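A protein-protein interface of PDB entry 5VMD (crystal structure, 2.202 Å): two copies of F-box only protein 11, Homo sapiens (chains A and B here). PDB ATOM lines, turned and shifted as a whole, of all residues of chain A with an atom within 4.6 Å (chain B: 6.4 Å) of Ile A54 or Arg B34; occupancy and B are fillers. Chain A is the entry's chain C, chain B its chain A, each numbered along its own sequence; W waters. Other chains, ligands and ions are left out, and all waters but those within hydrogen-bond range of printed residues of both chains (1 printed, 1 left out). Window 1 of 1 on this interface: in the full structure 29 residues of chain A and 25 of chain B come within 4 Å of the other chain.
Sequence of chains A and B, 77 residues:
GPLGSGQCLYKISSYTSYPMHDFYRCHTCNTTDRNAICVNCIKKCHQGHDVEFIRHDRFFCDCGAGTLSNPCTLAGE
The guanidinium group (NH1) of Arg A25 sits close to the guanidinium group (NH1) of Arg B34 (3.2 Å).
The guanidinium group (NH2) of Arg A34 lies close to the guanidinium group (NH1) of Arg B25 (3.2 Å).
The guanidinium group of Arg A34 sits close to the guanidinium group of Arg B34 (3.3 Å).
The side-chain carboxylate (OE1) of Glu A52 lies within salt-bridge range of the guanidinium group (NH1) of Arg B34 (2.5 Å).
NE of Arg B25 lies within hydrogen-bond range of O of Asn B35.
The guanidinium group (NH2) of Arg B25 sits close to the backbone carbonyl oxygen (O) of Arg B34, 3.2 Å away.
A ring nitrogen (NE2) of His A27 is in hydrogen-bond range of the side-chain carboxylate (OE1) of Glu A52, 2.7 Å away.
O of Arg A25 sits at hydrogen-bond distance from N of Glu A52, 2.7 Å away.
N of Phe A23 is in hydrogen-bond range of O of Ile A54, at 2.9 Å.
NH2 of Arg B34 touches CE1 of His A27, 3.8 Å away.
Arg B34 touches Ile A54 (NH1 to CD1, 3.3 Å).
Of chain B, only Arg B34 comes within 4 Å of Ile A54.
Of chain A, only Arg A25 (3.2 Å), His A27 (3.8 Å), Arg A34 (3.3 Å), Glu A52 (2.5 Å) and Ile A54 (3.3 Å) come within 4 Å of Arg B34.
Printed residues of chain B within 4 Å of Arg A25: Arg B34.
Printed residues of chain B within 4 Å of His A27: Arg B34.
Of the printed residues of chain B, Glu A52 touches Arg B34.
The nearest printed residue of chain A that does not touch Arg B34 is Phe A53 (5.9 Å).
Of the 11 printed residues of chain A, 5 touch a printed residue of chain B.
Among the printed residues, 6 pairs touch across the chains.
Arg A25 touches Arg B34, and with the chains exchanged Arg A34 touches Arg B25.
Arg B34 touches its own counterpart, Arg A34.
3 positions are printed for both chains.
Of the 6 pairs that touch across the chains among the printed residues, 3 have their exchanged pair printed and touching as well.
Water W1 bridges NH1 of Arg B25 (3.2 Å) and NH1 of Arg A25 (3.4 Å).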
ATOM      1  N   HIS A  21     -25.364  13.989 -21.983  1.00  0.00           N
ATOM      2  CA  HIS A  21     -25.643  14.907 -20.891  1.00  0.00           C
ATOM      3  C   HIS A  21     -25.378  14.203 -19.570  1.00  0.00           C
ATOM      4  O   HIS A  21     -25.387  12.969 -19.486  1.00  0.00           O
ATOM      5  CB  HIS A  21     -27.074  15.442 -20.953  1.00  0.00           C
ATOM      6  CG  HIS A  21     -28.119  14.388 -20.773  1.00  0.00           C
ATOM      7  ND1 HIS A  21     -28.706  13.736 -21.837  1.00  0.00           N
ATOM      8  CD2 HIS A  21     -28.693  13.880 -19.657  1.00  0.00           C
ATOM      9  CE1 HIS A  21     -29.593  12.870 -21.383  1.00  0.00           C
ATOM     10  NE2 HIS A  21     -29.605  12.938 -20.064  1.00  0.00           N
ATOM     11  N   ASP A  22     -25.164  15.012 -18.529  1.00  0.00           N
ATOM     12  CA  ASP A  22     -24.794  14.529 -17.205  1.00  0.00           C
ATOM     13  C   ASP A  22     -25.767  15.066 -16.169  1.00  0.00           C
ATOM     14  O   ASP A  22     -26.316  16.159 -16.312  1.00  0.00           O
ATOM     15  CB  ASP A  22     -23.380  14.970 -16.782  1.00  0.00           C
ATOM     16  CG  ASP A  22     -22.307  14.567 -17.769  1.00  0.00           C
ATOM     17  OD1 ASP A  22     -22.542  13.646 -18.575  1.00  0.00           O
ATOM     18  OD2 ASP A  22     -21.209  15.170 -17.720  1.00  0.00           O
ATOM     19  N   PHE A  23     -25.958  14.290 -15.113  1.00  0.00           N
ATOM     20  CA  PHE A  23     -26.819  14.697 -14.018  1.00  0.00           C
ATOM     21  C   PHE A  23     -26.444  13.848 -12.818  1.00  0.00           C
ATOM     22  O   PHE A  23     -25.541  13.010 -12.883  1.00  0.00           O
ATOM     23  CB  PHE A  23     -28.304  14.573 -14.381  1.00  0.00           C
ATOM     24  CG  PHE A  23     -28.752  13.164 -14.669  1.00  0.00           C
ATOM     25  CD1 PHE A  23     -28.528  12.588 -15.910  1.00  0.00           C
ATOM     26  CD2 PHE A  23     -29.424  12.426 -13.704  1.00  0.00           C
ATOM     27  CE1 PHE A  23     -28.956  11.294 -16.178  1.00  0.00           C
ATOM     28  CE2 PHE A  23     -29.852  11.139 -13.960  1.00  0.00           C
ATOM     29  CZ  PHE A  23     -29.620  10.568 -15.204  1.00  0.00           C
ATOM     30  N   ARG A  25     -27.833  11.643  -9.202  1.00  0.00           N
ATOM     31  CA  ARG A  25     -28.843  10.975  -8.401  1.00  0.00           C
ATOM     32  C   ARG A  25     -28.448  11.118  -6.938  1.00  0.00           C
ATOM     33  O   ARG A  25     -27.271  10.987  -6.592  1.00  0.00           O
ATOM     34  CB  ARG A  25     -28.949   9.495  -8.781  1.00  0.00           C
ATOM     35  CG  ARG A  25     -29.961   8.694  -7.989  1.00  0.00           C
ATOM     36  CD  ARG A  25     -30.564   7.590  -8.861  1.00  0.00           C
ATOM     37  NE  ARG A  25     -31.279   8.123 -10.016  1.00  0.00           N
ATOM     38  CZ  ARG A  25     -31.328   7.540 -11.210  1.00  0.00           C
ATOM     39  NH1 ARG A  25     -30.674   6.407 -11.434  1.00  0.00           N
ATOM     40  NH2 ARG A  25     -32.013   8.113 -12.191  1.00  0.00           N
ATOM     41  N   HIS A  27     -29.062   9.371  -3.472  1.00  0.00           N
ATOM     42  CA  HIS A  27     -29.613   8.226  -2.761  1.00  0.00           C
ATOM     43  C   HIS A  27     -30.005   8.546  -1.324  1.00  0.00           C
ATOM     44  O   HIS A  27     -30.744   7.765  -0.717  1.00  0.00           O
ATOM     45  CB  HIS A  27     -28.607   7.075  -2.809  1.00  0.00           C
ATOM     46  CG  HIS A  27     -28.206   6.707  -4.204  1.00  0.00           C
ATOM     47  ND1 HIS A  27     -28.993   5.924  -5.021  1.00  0.00           N
ATOM     48  CD2 HIS A  27     -27.128   7.059  -4.944  1.00  0.00           C
ATOM     49  CE1 HIS A  27     -28.405   5.789  -6.196  1.00  0.00           C
ATOM     50  NE2 HIS A  27     -27.272   6.468  -6.177  1.00  0.00           N
ATOM     51  N   ARG A  34     -36.008   6.527  -8.210  1.00  0.00           N
ATOM     52  CA  ARG A  34     -34.766   7.181  -8.595  1.00  0.00           C
ATOM     53  C   ARG A  34     -35.012   8.564  -9.196  1.00  0.00           C
ATOM     54  O   ARG A  34     -35.721   8.717 -10.198  1.00  0.00           O
ATOM     55  CB  ARG A  34     -34.003   6.286  -9.562  1.00  0.00           C
ATOM     56  CG  ARG A  34     -33.323   5.121  -8.866  1.00  0.00           C
ATOM     57  CD  ARG A  34     -32.323   4.451  -9.784  1.00  0.00           C
ATOM     58  NE  ARG A  34     -31.764   3.224  -9.211  1.00  0.00           N
ATOM     59  CZ  ARG A  34     -31.335   2.183  -9.926  1.00  0.00           C
ATOM     60  NH1 ARG A  34     -30.822   1.121  -9.316  1.00  0.00           N
ATOM     61  NH2 ARG A  34     -31.398   2.209 -11.254  1.00  0.00           N
ATOM     62  N   GLU A  52     -24.652  10.284  -6.653  1.00  0.00           N
ATOM     63  CA  GLU A  52     -24.095   9.461  -7.721  1.00  0.00           C
ATOM     64  C   GLU A  52     -24.099  10.231  -9.035  1.00  0.00           C
ATOM     65  O   GLU A  52     -25.126  10.789  -9.432  1.00  0.00           O
ATOM     66  CB  GLU A  52     -24.882   8.151  -7.889  1.00  0.00           C
ATOM     67  CG  GLU A  52     -24.383   7.285  -9.040  1.00  0.00           C
ATOM     68  CD  GLU A  52     -25.314   6.121  -9.361  1.00  0.00           C
ATOM     69  OE1 GLU A  52     -26.314   5.918  -8.639  1.00  0.00           O
ATOM     70  OE2 GLU A  52     -25.081   5.438 -10.381  1.00  0.00           O
ATOM     71  N   PHE A  53     -22.950  10.250  -9.706  1.00  0.00           N
ATOM     72  CA  PHE A  53     -22.824  10.858 -11.024  1.00  0.00           C
ATOM     73  C   PHE A  53     -23.324   9.913 -12.115  1.00  0.00           C
ATOM     74  O   PHE A  53     -23.047   8.715 -12.086  1.00  0.00           O
ATOM     75  CB  PHE A  53     -21.365  11.223 -11.287  1.00  0.00           C
ATOM     76  CG  PHE A  53     -21.104  11.749 -12.668  1.00  0.00           C
ATOM     77  CD1 PHE A  53     -20.745  10.881 -13.694  1.00  0.00           C
ATOM     78  CD2 PHE A  53     -21.201  13.101 -12.943  1.00  0.00           C
ATOM     79  CE1 PHE A  53     -20.499  11.355 -14.969  1.00  0.00           C
ATOM     80  CE2 PHE A  53     -20.953  13.585 -14.218  1.00  0.00           C
ATOM     81  CZ  PHE A  53     -20.600  12.712 -15.233  1.00  0.00           C
ATOM     82  N   ILE A  54     -24.080  10.460 -13.069  1.00  0.00           N
ATOM     83  CA  ILE A  54     -24.641   9.689 -14.172  1.00  0.00           C
ATOM     84  C   ILE A  54     -24.434  10.456 -15.470  1.00  0.00           C
ATOM     85  O   ILE A  54     -24.743  11.650 -15.552  1.00  0.00           O
ATOM     86  CB  ILE A  54     -26.135   9.383 -13.968  1.00  0.00           C
ATOM     87  CG1 ILE A  54     -26.334   8.535 -12.713  1.00  0.00           C
ATOM     88  CG2 ILE A  54     -26.682   8.644 -15.181  1.00  0.00           C
ATOM     89  CD1 ILE A  54     -27.782   8.205 -12.425  1.00  0.00           C
ATOM     90  N   ARG A  55     -23.896   9.774 -16.476  1.00  0.00           N
ATOM     91  CA  ARG A  55     -23.742  10.304 -17.822  1.00  0.00           C
ATOM     92  C   ARG A  55     -24.555   9.459 -18.798  1.00  0.00           C
ATOM     93  O   ARG A  55     -24.421   8.230 -18.818  1.00  0.00           O
ATOM     94  CB  ARG A  55     -22.270  10.318 -18.227  1.00  0.00           C
ATOM     95  CG  ARG A  55     -22.041  10.695 -19.669  1.00  0.00           C
ATOM     96  CD  ARG A  55     -20.588  10.989 -19.894  1.00  0.00           C
ATOM     97  NE  ARG A  55     -20.196  12.227 -19.227  1.00  0.00           N
ATOM     98  CZ  ARG A  55     -18.936  12.602 -19.049  1.00  0.00           C
ATOM     99  NH1 ARG A  55     -17.948  11.824 -19.477  1.00  0.00           N
ATOM    100  NH2 ARG A  55     -18.668  13.745 -18.441  1.00  0.00           N
ATOM    101  N   HIS A  56     -25.368  10.125 -19.621  1.00  0.00           N
ATOM    102  CA  HIS A  56     -26.267   9.492 -20.583  1.00  0.00           C
ATOM    103  C   HIS A  56     -25.824   9.805 -22.007  1.00  0.00           C
ATOM    104  O   HIS A  56     -25.584  10.969 -22.343  1.00  0.00           O
ATOM    105  CB  HIS A  56     -27.714   9.984 -20.406  1.00  0.00           C
ATOM    106  CG  HIS A  56     -28.481   9.279 -19.332  1.00  0.00           C
ATOM    107  ND1 HIS A  56     -29.772   9.629 -18.992  1.00  0.00           N
ATOM    108  CD2 HIS A  56     -28.146   8.250 -18.518  1.00  0.00           C
ATOM    109  CE1 HIS A  56     -30.201   8.845 -18.021  1.00  0.00           C
ATOM    110  NE2 HIS A  56     -29.233   7.998 -17.714  1.00  0.00           N
ATOM    111  N   PHE B  23     -35.578   5.267 -23.100  1.00  0.00           N
ATOM    112  CA  PHE B  23     -34.858   4.016 -23.261  1.00  0.00           C
ATOM    113  C   PHE B  23     -35.464   3.002 -22.306  1.00  0.00           C
ATOM    114  O   PHE B  23     -36.412   3.295 -21.570  1.00  0.00           O
ATOM    115  CB  PHE B  23     -33.357   4.205 -23.013  1.00  0.00           C
ATOM    116  CG  PHE B  23     -33.027   4.718 -21.637  1.00  0.00           C
ATOM    117  CD1 PHE B  23     -33.086   6.077 -21.355  1.00  0.00           C
ATOM    118  CD2 PHE B  23     -32.668   3.847 -20.621  1.00  0.00           C
ATOM    119  CE1 PHE B  23     -32.767   6.557 -20.074  1.00  0.00           C
ATOM    120  CE2 PHE B  23     -32.361   4.321 -19.350  1.00  0.00           C
ATOM    121  CZ  PHE B  23     -32.415   5.681 -19.079  1.00  0.00           C
ATOM    122  N   ARG B  25     -34.659  -0.257 -19.429  1.00  0.00           N
ATOM    123  CA  ARG B  25     -33.783  -0.997 -18.546  1.00  0.00           C
ATOM    124  C   ARG B  25     -34.318  -2.416 -18.511  1.00  0.00           C
ATOM    125  O   ARG B  25     -35.535  -2.620 -18.425  1.00  0.00           O
ATOM    126  CB  ARG B  25     -33.762  -0.388 -17.139  1.00  0.00           C
ATOM    127  CG  ARG B  25     -32.869  -1.144 -16.155  1.00  0.00           C
ATOM    128  CD  ARG B  25     -32.231  -0.187 -15.176  1.00  0.00           C
ATOM    129  NE  ARG B  25     -31.437   0.795 -15.899  1.00  0.00           N
ATOM    130  CZ  ARG B  25     -31.281   2.055 -15.517  1.00  0.00           C
ATOM    131  NH1 ARG B  25     -31.854   2.487 -14.402  1.00  0.00           N
ATOM    132  NH2 ARG B  25     -30.556   2.883 -16.255  1.00  0.00           N
ATOM    133  N   THR B  32     -25.054  -6.284 -16.151  1.00  0.00           N
ATOM    134  CA  THR B  32     -24.655  -4.891 -16.323  1.00  0.00           C
ATOM    135  C   THR B  32     -25.671  -4.037 -15.577  1.00  0.00           C
ATOM    136  O   THR B  32     -26.835  -3.946 -15.986  1.00  0.00           O
ATOM    137  CB  THR B  32     -24.594  -4.505 -17.800  1.00  0.00           C
ATOM    138  OG1 THR B  32     -23.496  -5.181 -18.424  1.00  0.00           O
ATOM    139  CG2 THR B  32     -24.430  -2.997 -17.959  1.00  0.00           C
ATOM    140  N   ASP B  33     -25.231  -3.419 -14.486  1.00  0.00           N
ATOM    141  CA  ASP B  33     -26.143  -2.697 -13.614  1.00  0.00           C
ATOM    142  C   ASP B  33     -26.568  -1.372 -14.241  1.00  0.00           C
ATOM    143  O   ASP B  33     -25.761  -0.655 -14.841  1.00  0.00           O
ATOM    144  CB  ASP B  33     -25.484  -2.455 -12.257  1.00  0.00           C
ATOM    145  CG  ASP B  33     -26.454  -1.932 -11.224  1.00  0.00           C
ATOM    146  OD1 ASP B  33     -26.043  -1.077 -10.411  1.00  0.00           O
ATOM    147  OD2 ASP B  33     -27.623  -2.374 -11.224  1.00  0.00           O
ATOM    148  N   ARG B  34     -27.852  -1.048 -14.107  1.00  0.00           N
ATOM    149  CA  ARG B  34     -28.358   0.228 -14.597  1.00  0.00           C
ATOM    150  C   ARG B  34     -28.159   0.336 -16.110  1.00  0.00           C
ATOM    151  O   ARG B  34     -27.751   1.377 -16.633  1.00  0.00           O
ATOM    152  CB  ARG B  34     -27.687   1.388 -13.855  1.00  0.00           C
ATOM    153  CG  ARG B  34     -28.396   2.728 -13.994  1.00  0.00           C
ATOM    154  CD  ARG B  34     -27.881   3.737 -12.973  1.00  0.00           C
ATOM    155  NE  ARG B  34     -28.252   3.332 -11.611  1.00  0.00           N
ATOM    156  CZ  ARG B  34     -28.157   4.124 -10.544  1.00  0.00           C
ATOM    157  NH1 ARG B  34     -27.705   5.352 -10.693  1.00  0.00           N
ATOM    158  NH2 ARG B  34     -28.504   3.710  -9.332  1.00  0.00           N
ATOM    159  N   ASN B  35     -28.439  -0.759 -16.821  1.00  0.00           N
ATOM    160  CA  ASN B  35     -28.191  -0.786 -18.254  1.00  0.00           C
ATOM    161  C   ASN B  35     -29.163   0.142 -18.988  1.00  0.00           C
ATOM    162  O   ASN B  35     -30.166   0.603 -18.440  1.00  0.00           O
ATOM    163  CB  ASN B  35     -28.296  -2.221 -18.792  1.00  0.00           C
ATOM    164  CG  ASN B  35     -29.637  -2.881 -18.487  1.00  0.00           C
ATOM    165  OD1 ASN B  35     -30.701  -2.335 -18.769  1.00  0.00           O
ATOM    166  ND2 ASN B  35     -29.584  -4.067 -17.895  1.00  0.00           N
ATOM    167  N   ALA B  36     -28.858   0.392 -20.261  1.00  0.00           N
ATOM    168  CA  ALA B  36     -29.702   1.192 -21.136  1.00  0.00           C
ATOM    169  C   ALA B  36     -29.807   0.499 -22.487  1.00  0.00           C
ATOM    170  O   ALA B  36     -28.790   0.205 -23.123  1.00  0.00           O
ATOM    171  CB  ALA B  36     -29.146   2.612 -21.296  1.00  0.00           C
HETATM  172  O   HOH W   1     -31.465   5.666 -14.638  1.00  0.00           O
